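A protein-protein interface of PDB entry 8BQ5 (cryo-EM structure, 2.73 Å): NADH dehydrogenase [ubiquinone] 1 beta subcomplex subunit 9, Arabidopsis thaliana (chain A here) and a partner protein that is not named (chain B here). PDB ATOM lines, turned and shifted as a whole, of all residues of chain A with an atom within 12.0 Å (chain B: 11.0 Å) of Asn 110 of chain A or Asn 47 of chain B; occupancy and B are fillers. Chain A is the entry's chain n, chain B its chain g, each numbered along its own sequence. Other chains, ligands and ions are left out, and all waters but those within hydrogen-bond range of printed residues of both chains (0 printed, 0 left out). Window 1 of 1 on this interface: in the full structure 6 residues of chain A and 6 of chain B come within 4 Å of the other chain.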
ATOM      1  N   ILE A 105     -24.571  -8.941 -24.862  1.00  0.00           N
ATOM      2  CA  ILE A 105     -24.067  -8.323 -23.643  1.00  0.00           C
ATOM      3  C   ILE A 105     -25.259  -7.848 -22.826  1.00  0.00           C
ATOM      4  O   ILE A 105     -26.163  -7.192 -23.353  1.00  0.00           O
ATOM      5  CB  ILE A 105     -23.110  -7.161 -23.950  1.00  0.00           C
ATOM      6  CG1 ILE A 105     -21.907  -7.652 -24.757  1.00  0.00           C
ATOM      7  CG2 ILE A 105     -22.649  -6.499 -22.659  1.00  0.00           C
ATOM      8  CD1 ILE A 105     -21.245  -8.881 -24.193  1.00  0.00           C
ATOM      9  N   GLU A 106     -25.263  -8.182 -21.543  1.00  0.00           N
ATOM     10  CA  GLU A 106     -26.325  -7.793 -20.630  1.00  0.00           C
ATOM     11  C   GLU A 106     -25.756  -6.944 -19.505  1.00  0.00           C
ATOM     12  O   GLU A 106     -24.658  -7.208 -19.006  1.00  0.00           O
ATOM     13  CB  GLU A 106     -27.038  -9.027 -20.074  1.00  0.00           C
ATOM     14  CG  GLU A 106     -26.882 -10.242 -20.965  1.00  0.00           C
ATOM     15  CD  GLU A 106     -27.729 -11.416 -20.536  1.00  0.00           C
ATOM     16  OE1 GLU A 106     -27.291 -12.195 -19.679  1.00  0.00           O
ATOM     17  OE2 GLU A 106     -28.841 -11.580 -21.063  1.00  0.00           O
ATOM     18  N   ILE A 107     -26.498  -5.908 -19.129  1.00  0.00           N
ATOM     19  CA  ILE A 107     -26.132  -5.019 -18.035  1.00  0.00           C
ATOM     20  C   ILE A 107     -27.128  -5.239 -16.905  1.00  0.00           C
ATOM     21  O   ILE A 107     -28.339  -5.079 -17.099  1.00  0.00           O
ATOM     22  CB  ILE A 107     -26.123  -3.547 -18.485  1.00  0.00           C
ATOM     23  CG1 ILE A 107     -25.187  -3.348 -19.680  1.00  0.00           C
ATOM     24  CG2 ILE A 107     -25.723  -2.641 -17.335  1.00  0.00           C
ATOM     25  CD1 ILE A 107     -23.784  -3.866 -19.468  1.00  0.00           C
ATOM     26  N   VAL A 108     -26.621  -5.607 -15.731  1.00  0.00           N
ATOM     27  CA  VAL A 108     -27.451  -5.912 -14.569  1.00  0.00           C
ATOM     28  C   VAL A 108     -27.610  -4.660 -13.725  1.00  0.00           C
ATOM     29  O   VAL A 108     -26.634  -3.946 -13.456  1.00  0.00           O
ATOM     30  CB  VAL A 108     -26.852  -7.055 -13.731  1.00  0.00           C
ATOM     31  CG1 VAL A 108     -27.814  -7.461 -12.627  1.00  0.00           C
ATOM     32  CG2 VAL A 108     -26.527  -8.239 -14.609  1.00  0.00           C
ATOM     33  N   TYR A 109     -28.839  -4.390 -13.306  1.00  0.00           N
ATOM     34  CA  TYR A 109     -29.126  -3.324 -12.361  1.00  0.00           C
ATOM     35  C   TYR A 109     -29.386  -3.931 -10.989  1.00  0.00           C
ATOM     36  O   TYR A 109     -29.626  -5.134 -10.864  1.00  0.00           O
ATOM     37  CB  TYR A 109     -30.339  -2.507 -12.804  1.00  0.00           C
ATOM     38  CG  TYR A 109     -30.140  -1.747 -14.090  1.00  0.00           C
ATOM     39  CD1 TYR A 109     -28.899  -1.227 -14.432  1.00  0.00           C
ATOM     40  CD2 TYR A 109     -31.195  -1.553 -14.967  1.00  0.00           C
ATOM     41  CE1 TYR A 109     -28.720  -0.533 -15.611  1.00  0.00           C
ATOM     42  CE2 TYR A 109     -31.028  -0.863 -16.142  1.00  0.00           C
ATOM     43  CZ  TYR A 109     -29.790  -0.355 -16.462  1.00  0.00           C
ATOM     44  OH  TYR A 109     -29.627   0.335 -17.639  1.00  0.00           O
ATOM     45  N   ASN A 110     -29.328  -3.084  -9.960  1.00  0.00           N
ATOM     46  CA  ASN A 110     -29.684  -3.473  -8.593  1.00  0.00           C
ATOM     47  C   ASN A 110     -28.885  -4.682  -8.111  1.00  0.00           C
ATOM     48  O   ASN A 110     -29.436  -5.616  -7.523  1.00  0.00           O
ATOM     49  CB  ASN A 110     -31.185  -3.740  -8.474  1.00  0.00           C
ATOM     50  CG  ASN A 110     -32.024  -2.589  -8.978  1.00  0.00           C
ATOM     51  OD1 ASN A 110     -31.899  -1.460  -8.503  1.00  0.00           O
ATOM     52  ND2 ASN A 110     -32.891  -2.869  -9.941  1.00  0.00           N
ATOM     53  N   TYR A 111     -27.580  -4.673  -8.357  1.00  0.00           N
ATOM     54  CA  TYR A 111     -26.726  -5.741  -7.864  1.00  0.00           C
ATOM     55  C   TYR A 111     -26.125  -5.365  -6.514  1.00  0.00           C
ATOM     56  O   TYR A 111     -25.857  -4.194  -6.233  1.00  0.00           O
ATOM     57  CB  TYR A 111     -25.610  -6.050  -8.862  1.00  0.00           C
ATOM     58  CG  TYR A 111     -24.688  -7.156  -8.406  1.00  0.00           C
ATOM     59  CD1 TYR A 111     -25.087  -8.483  -8.465  1.00  0.00           C
ATOM     60  CD2 TYR A 111     -23.428  -6.872  -7.898  1.00  0.00           C
ATOM     61  CE1 TYR A 111     -24.254  -9.498  -8.043  1.00  0.00           C
ATOM     62  CE2 TYR A 111     -22.588  -7.881  -7.470  1.00  0.00           C
ATOM     63  CZ  TYR A 111     -23.007  -9.192  -7.546  1.00  0.00           C
ATOM     64  OH  TYR A 111     -22.179 -10.205  -7.124  1.00  0.00           O
ATOM     65  N   GLY A 112     -25.922  -6.374  -5.673  1.00  0.00           N
ATOM     66  CA  GLY A 112     -25.279  -6.155  -4.391  1.00  0.00           C
ATOM     67  C   GLY A 112     -26.156  -5.521  -3.337  1.00  0.00           C
ATOM     68  O   GLY A 112     -25.639  -4.883  -2.415  1.00  0.00           O
ATOM     69  N   LEU A 113     -27.474  -5.665  -3.454  1.00  0.00           N
ATOM     70  CA  LEU A 113     -28.383  -5.146  -2.444  1.00  0.00           C
ATOM     71  C   LEU A 113     -28.231  -5.913  -1.135  1.00  0.00           C
ATOM     72  O   LEU A 113     -27.845  -7.085  -1.115  1.00  0.00           O
ATOM     73  CB  LEU A 113     -29.829  -5.231  -2.929  1.00  0.00           C
ATOM     74  CG  LEU A 113     -30.209  -4.307  -4.086  1.00  0.00           C
ATOM     75  CD1 LEU A 113     -31.581  -4.668  -4.624  1.00  0.00           C
ATOM     76  CD2 LEU A 113     -30.179  -2.862  -3.625  1.00  0.00           C
ATOM     77  N   GLU A 114     -28.543  -5.234  -0.029  1.00  0.00           N
ATOM     78  CA  GLU A 114     -28.373  -5.848   1.283  1.00  0.00           C
ATOM     79  C   GLU A 114     -29.375  -6.972   1.525  1.00  0.00           C
ATOM     80  O   GLU A 114     -29.072  -7.917   2.262  1.00  0.00           O
ATOM     81  CB  GLU A 114     -28.463  -4.783   2.379  1.00  0.00           C
ATOM     82  CG  GLU A 114     -29.624  -3.814   2.238  1.00  0.00           C
ATOM     83  CD  GLU A 114     -29.813  -2.942   3.469  1.00  0.00           C
ATOM     84  OE1 GLU A 114     -28.857  -2.807   4.261  1.00  0.00           O
ATOM     85  OE2 GLU A 114     -30.917  -2.387   3.641  1.00  0.00           O
ATOM     86  N   ASP A 115     -30.558  -6.902   0.922  1.00  0.00           N
ATOM     87  CA  ASP A 115     -31.528  -7.986   1.060  1.00  0.00           C
ATOM     88  C   ASP A 115     -31.270  -9.082   0.030  1.00  0.00           C
ATOM     89  O   ASP A 115     -32.199  -9.732  -0.445  1.00  0.00           O
ATOM     90  CB  ASP A 115     -32.961  -7.470   0.920  1.00  0.00           C
ATOM     91  CG  ASP A 115     -33.418  -6.682   2.132  1.00  0.00           C
ATOM     92  OD1 ASP A 115     -32.716  -6.715   3.163  1.00  0.00           O
ATOM     93  OD2 ASP A 115     -34.491  -6.047   2.059  1.00  0.00           O
ATOM     94  N   LYS B  42     -28.156   7.881 -20.663  1.00  0.00           N
ATOM     95  CA  LYS B  42     -28.073   6.446 -20.883  1.00  0.00           C
ATOM     96  C   LYS B  42     -27.584   5.756 -19.616  1.00  0.00           C
ATOM     97  O   LYS B  42     -26.644   6.216 -18.963  1.00  0.00           O
ATOM     98  CB  LYS B  42     -27.142   6.131 -22.053  1.00  0.00           C
ATOM     99  CG  LYS B  42     -25.793   6.812 -21.978  1.00  0.00           C
ATOM    100  CD  LYS B  42     -24.818   6.194 -22.959  1.00  0.00           C
ATOM    101  CE  LYS B  42     -25.056   6.713 -24.364  1.00  0.00           C
ATOM    102  NZ  LYS B  42     -24.649   8.138 -24.513  1.00  0.00           N
ATOM    103  N   GLY B  43     -28.243   4.656 -19.260  1.00  0.00           N
ATOM    104  CA  GLY B  43     -27.940   3.963 -18.026  1.00  0.00           C
ATOM    105  C   GLY B  43     -28.475   4.705 -16.816  1.00  0.00           C
ATOM    106  O   GLY B  43     -29.170   5.717 -16.915  1.00  0.00           O
ATOM    107  N   TYR B  44     -28.134   4.181 -15.642  1.00  0.00           N
ATOM    108  CA  TYR B  44     -28.522   4.785 -14.377  1.00  0.00           C
ATOM    109  C   TYR B  44     -27.296   4.951 -13.495  1.00  0.00           C
ATOM    110  O   TYR B  44     -26.398   4.104 -13.501  1.00  0.00           O
ATOM    111  CB  TYR B  44     -29.576   3.943 -13.653  1.00  0.00           C
ATOM    112  CG  TYR B  44     -30.863   3.802 -14.428  1.00  0.00           C
ATOM    113  CD1 TYR B  44     -31.716   4.884 -14.594  1.00  0.00           C
ATOM    114  CD2 TYR B  44     -31.218   2.591 -15.005  1.00  0.00           C
ATOM    115  CE1 TYR B  44     -32.889   4.762 -15.308  1.00  0.00           C
ATOM    116  CE2 TYR B  44     -32.389   2.460 -15.718  1.00  0.00           C
ATOM    117  CZ  TYR B  44     -33.221   3.547 -15.867  1.00  0.00           C
ATOM    118  OH  TYR B  44     -34.389   3.420 -16.579  1.00  0.00           O
ATOM    119  N   PHE B  45     -27.266   6.044 -12.739  1.00  0.00           N
ATOM    120  CA  PHE B  45     -26.156   6.302 -11.833  1.00  0.00           C
ATOM    121  C   PHE B  45     -26.066   5.200 -10.786  1.00  0.00           C
ATOM    122  O   PHE B  45     -27.017   4.968 -10.034  1.00  0.00           O
ATOM    123  CB  PHE B  45     -26.334   7.664 -11.166  1.00  0.00           C
ATOM    124  CG  PHE B  45     -25.213   8.037 -10.243  1.00  0.00           C
ATOM    125  CD1 PHE B  45     -23.900   7.987 -10.674  1.00  0.00           C
ATOM    126  CD2 PHE B  45     -25.472   8.450  -8.948  1.00  0.00           C
ATOM    127  CE1 PHE B  45     -22.863   8.333  -9.831  1.00  0.00           C
ATOM    128  CE2 PHE B  45     -24.441   8.800  -8.101  1.00  0.00           C
ATOM    129  CZ  PHE B  45     -23.133   8.740  -8.543  1.00  0.00           C
ATOM    130  N   MET B  46     -24.920   4.517 -10.750  1.00  0.00           N
ATOM    131  CA  MET B  46     -24.673   3.415  -9.818  1.00  0.00           C
ATOM    132  C   MET B  46     -25.655   2.264 -10.016  1.00  0.00           C
ATOM    133  O   MET B  46     -25.943   1.512  -9.082  1.00  0.00           O
ATOM    134  CB  MET B  46     -24.676   3.903  -8.366  1.00  0.00           C
ATOM    135  CG  MET B  46     -23.470   4.769  -8.021  1.00  0.00           C
ATOM    136  SD  MET B  46     -23.695   5.880  -6.619  1.00  0.00           S
ATOM    137  CE  MET B  46     -25.241   5.287  -5.952  1.00  0.00           C
ATOM    138  N   ASN B  47     -26.176   2.135 -11.239  1.00  0.00           N
ATOM    139  CA  ASN B  47     -26.904   0.949 -11.696  1.00  0.00           C
ATOM    140  C   ASN B  47     -28.051   0.562 -10.768  1.00  0.00           C
ATOM    141  O   ASN B  47     -28.278  -0.622 -10.509  1.00  0.00           O
ATOM    142  CB  ASN B  47     -25.955  -0.236 -11.882  1.00  0.00           C
ATOM    143  CG  ASN B  47     -25.169  -0.148 -13.170  1.00  0.00           C
ATOM    144  OD1 ASN B  47     -24.091   0.441 -13.216  1.00  0.00           O
ATOM    145  ND2 ASN B  47     -25.698  -0.754 -14.222  1.00  0.00           N
ATOM    146  N   ARG B  48     -28.789   1.544 -10.265  1.00  0.00           N
ATOM    147  CA  ARG B  48     -29.997   1.297  -9.492  1.00  0.00           C
ATOM    148  C   ARG B  48     -31.197   1.822 -10.266  1.00  0.00           C
ATOM    149  O   ARG B  48     -31.193   2.968 -10.726  1.00  0.00           O
ATOM    150  CB  ARG B  48     -29.915   1.953  -8.112  1.00  0.00           C
ATOM    151  CG  ARG B  48     -29.434   3.386  -8.135  1.00  0.00           C
ATOM    152  CD  ARG B  48     -29.758   4.089  -6.834  1.00  0.00           C
ATOM    153  NE  ARG B  48     -28.929   3.618  -5.732  1.00  0.00           N
ATOM    154  CZ  ARG B  48     -28.348   4.413  -4.845  1.00  0.00           C
ATOM    155  NH1 ARG B  48     -28.479   5.728  -4.906  1.00  0.00           N
ATOM    156  NH2 ARG B  48     -27.615   3.876  -3.874  1.00  0.00           N
ATOM    157  N   THR B  49     -32.210   0.976 -10.429  1.00  0.00           N
ATOM    158  CA  THR B  49     -33.427   1.400 -11.099  1.00  0.00           C
ATOM    159  C   THR B  49     -34.154   2.447 -10.256  1.00  0.00           C
ATOM    160  O   THR B  49     -34.253   2.313  -9.034  1.00  0.00           O
ATOM    161  CB  THR B  49     -34.348   0.211 -11.350  1.00  0.00           C
ATOM    162  OG1 THR B  49     -34.615  -0.456 -10.110  1.00  0.00           O
ATOM    163  CG2 THR B  49     -33.707  -0.764 -12.323  1.00  0.00           C
ATOM    164  N   PRO B  50     -34.661   3.502 -10.886  1.00  0.00           N
ATOM    165  CA  PRO B  50     -35.353   4.555 -10.141  1.00  0.00           C
ATOM    166  C   PRO B  50     -36.602   4.022  -9.463  1.00  0.00           C
ATOM    167  O   PRO B  50     -37.215   3.054  -9.937  1.00  0.00           O
ATOM    168  CB  PRO B  50     -35.701   5.575 -11.234  1.00  0.00           C
ATOM    169  CG  PRO B  50     -34.596   5.401 -12.219  1.00  0.00           C
ATOM    170  CD  PRO B  50     -34.441   3.901 -12.285  1.00  0.00           C
ATOM    171  N   PRO B  51     -37.004   4.617  -8.344  1.00  0.00           N
ATOM    172  CA  PRO B  51     -38.242   4.189  -7.688  1.00  0.00           C
ATOM    173  C   PRO B  51     -39.462   4.600  -8.500  1.00  0.00           C
ATOM    174  O   PRO B  51     -39.368   5.311  -9.503  1.00  0.00           O
ATOM    175  CB  PRO B  51     -38.205   4.905  -6.335  1.00  0.00           C
ATOM    176  CG  PRO B  51     -37.302   6.072  -6.537  1.00  0.00           C
ATOM    177  CD  PRO B  51     -36.343   5.728  -7.638  1.00  0.00           C
ATOM    178  N   ALA B  52     -40.623   4.130  -8.050  1.00  0.00           N
ATOM    179  CA  ALA B  52     -41.861   4.432  -8.747  1.00  0.00           C
ATOM    180  C   ALA B  52     -42.127   5.937  -8.719  1.00  0.00           C
ATOM    181  O   ALA B  52     -41.792   6.614  -7.743  1.00  0.00           O
ATOM    182  CB  ALA B  52     -43.027   3.675  -8.117  1.00  0.00           C
ATOM    183  N   ARG B  57     -36.407   6.831  -3.149  1.00  0.00           N
ATOM    184  CA  ARG B  57     -35.558   5.673  -2.913  1.00  0.00           C
ATOM    185  C   ARG B  57     -35.474   5.373  -1.422  1.00  0.00           C
ATOM    186  O   ARG B  57     -35.408   6.281  -0.589  1.00  0.00           O
ATOM    187  CB  ARG B  57     -34.162   5.920  -3.482  1.00  0.00           C
ATOM    188  CG  ARG B  57     -33.137   4.850  -3.144  1.00  0.00           C
ATOM    189  CD  ARG B  57     -31.770   5.212  -3.698  1.00  0.00           C
ATOM    190  NE  ARG B  57     -31.118   6.257  -2.917  1.00  0.00           N
ATOM    191  CZ  ARG B  57     -30.257   6.027  -1.936  1.00  0.00           C
ATOM    192  NH1 ARG B  57     -29.920   4.797  -1.586  1.00  0.00           N
ATOM    193  NH2 ARG B  57     -29.720   7.058  -1.290  1.00  0.00           N
ATOM    194  N   LYS B  58     -35.497   4.087  -1.088  1.00  0.00           N
ATOM    195  CA  LYS B  58     -35.308   3.660   0.289  1.00  0.00           C
ATOM    196  C   LYS B  58     -33.819   3.576   0.596  1.00  0.00           C
ATOM    197  O   LYS B  58     -33.060   2.934  -0.138  1.00  0.00           O
ATOM    198  CB  LYS B  58     -35.983   2.311   0.530  1.00  0.00           C
ATOM    199  CG  LYS B  58     -36.498   2.116   1.945  1.00  0.00           C
ATOM    200  CD  LYS B  58     -36.234   0.702   2.434  1.00  0.00           C
ATOM    201  CE  LYS B  58     -36.342   0.607   3.946  1.00  0.00           C
ATOM    202  NZ  LYS B  58     -35.604  -0.573   4.482  1.00  0.00           N
ATOM    203  N   GLU B  60     -30.577   2.263   2.235  1.00  0.00           N
ATOM    204  CA  GLU B  60     -30.099   1.051   2.877  1.00  0.00           C
ATOM    205  C   GLU B  60     -29.580   1.364   4.277  1.00  0.00           C
ATOM    206  O   GLU B  60     -29.262   2.508   4.613  1.00  0.00           O
ATOM    207  CB  GLU B  60     -29.005   0.384   2.045  1.00  0.00           C
ATOM    208  CG  GLU B  60     -29.356   0.201   0.586  1.00  0.00           C
ATOM    209  CD  GLU B  60     -29.005  -1.181   0.074  1.00  0.00           C
ATOM    210  OE1 GLU B  60     -29.924  -1.899  -0.372  1.00  0.00           O
ATOM    211  OE2 GLU B  60     -27.814  -1.553   0.121  1.00  0.00           O
ATOM    212  N   GLU B  63     -26.370   3.505   5.002  1.00  0.00           N
ATOM    213  CA  GLU B  63     -26.193   4.847   4.452  1.00  0.00           C
ATOM    214  C   GLU B  63     -26.179   5.909   5.545  1.00  0.00           C
ATOM    215  O   GLU B  63     -25.276   6.750   5.596  1.00  0.00           O
ATOM    216  CB  GLU B  63     -27.288   5.141   3.427  1.00  0.00           C
ATOM    217  CG  GLU B  63     -27.293   4.182   2.255  1.00  0.00           C
ATOM    218  CD  GLU B  63     -27.804   4.817   0.981  1.00  0.00           C
ATOM    219  OE1 GLU B  63     -27.419   5.969   0.689  1.00  0.00           O
ATOM    220  OE2 GLU B  63     -28.597   4.163   0.273  1.00  0.00           O
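The side-chain amide nitrogen (ND2) of Asn 110 of chain A sits at hydrogen-bond distance from the side-chain hydroxyl (OG1) of Thr 49 of chain B (3.0 Å). N of Asn 110 of chain A lies within hydrogen-bond range of O of Asn 47 of chain B, 2.7 Å away. The side-chain amide nitrogen (ND2) of Asn 47 of chain B is in hydrogen-bond range of the backbone carbonyl oxygen (O) of Val 108 of chain A (3.4 Å).
The side-chain carboxylate (OE2) of Glu 63 of chain B is in hydrogen-bond range of the backbone NH (N) of Glu 60 of chain B (3.4 Å).
Among the printed residues, pairs that only touch across the chains: Tyr 109 of chain A with Asn 47 of chain B, Glu 114 of chain A with Glu 60 of chain B, Leu 113 of chain A with Glu 60 of chain B, Asn 110 of chain A with Arg 48 of chain B, Tyr 109 of chain A with Tyr 44 of chain B, Ile 107 of chain A with Asn 47 of chain B and Tyr 109 of chain A with Thr 49 of chain B.
Of the printed residues of chain B, Val 108 of chain A touches Asn 47. Of chain B, only Asn 47 (2.7 Å), Arg 48 (3.5 Å) and Thr 49 (3.0 Å) come within 4 Å of Asn 110 of chain A. No residue of chain B comes within 4 Å of Gly 112 of chain A. Of chain B, only Glu 60 comes within 4 Å of Leu 113 of chain A. No residue of chain A comes within 4 Å of Phe 45 of chain B. No residue of chain A comes within 4 Å of Met 46 of chain B. Of the printed residues of chain A, Asn 47 of chain B touches Ile 107 (3.6 Å), Val 108 (3.4 Å), Tyr 109 (3.2 Å) and Asn 110 (2.7 Å). Arg 48 of chain B touches one residue of chain A. Thr 49 of chain B touches just these residues of chain A: Tyr 109 and Asn 110. Printed residues of chain A within 4 Å of Glu 60 of chain B: Leu 113 (3.4 Å) and Glu 114 (3.3 Å). The nearest residue of chain B that does not touch Asn 110 of chain A is Met 46 of chain B (5.8 Å). The nearest residue of chain A that does not touch Asn 47 of chain B is Tyr 111 of chain A (4.6 Å). The nearest printed residue of chain B that does not touch Glu 114 of chain A is Lys 58 of chain B (5.1 Å).
Hydrophobic or aromatic side chains of chain B that line the printed part of chain A: Tyr 44. Among the printed residues, 10 pairs touch across the chains. Among the printed residues, no Asp or Glu carboxylate lies within 4 Å of a Lys or Arg side-chain nitrogen of the other chain.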
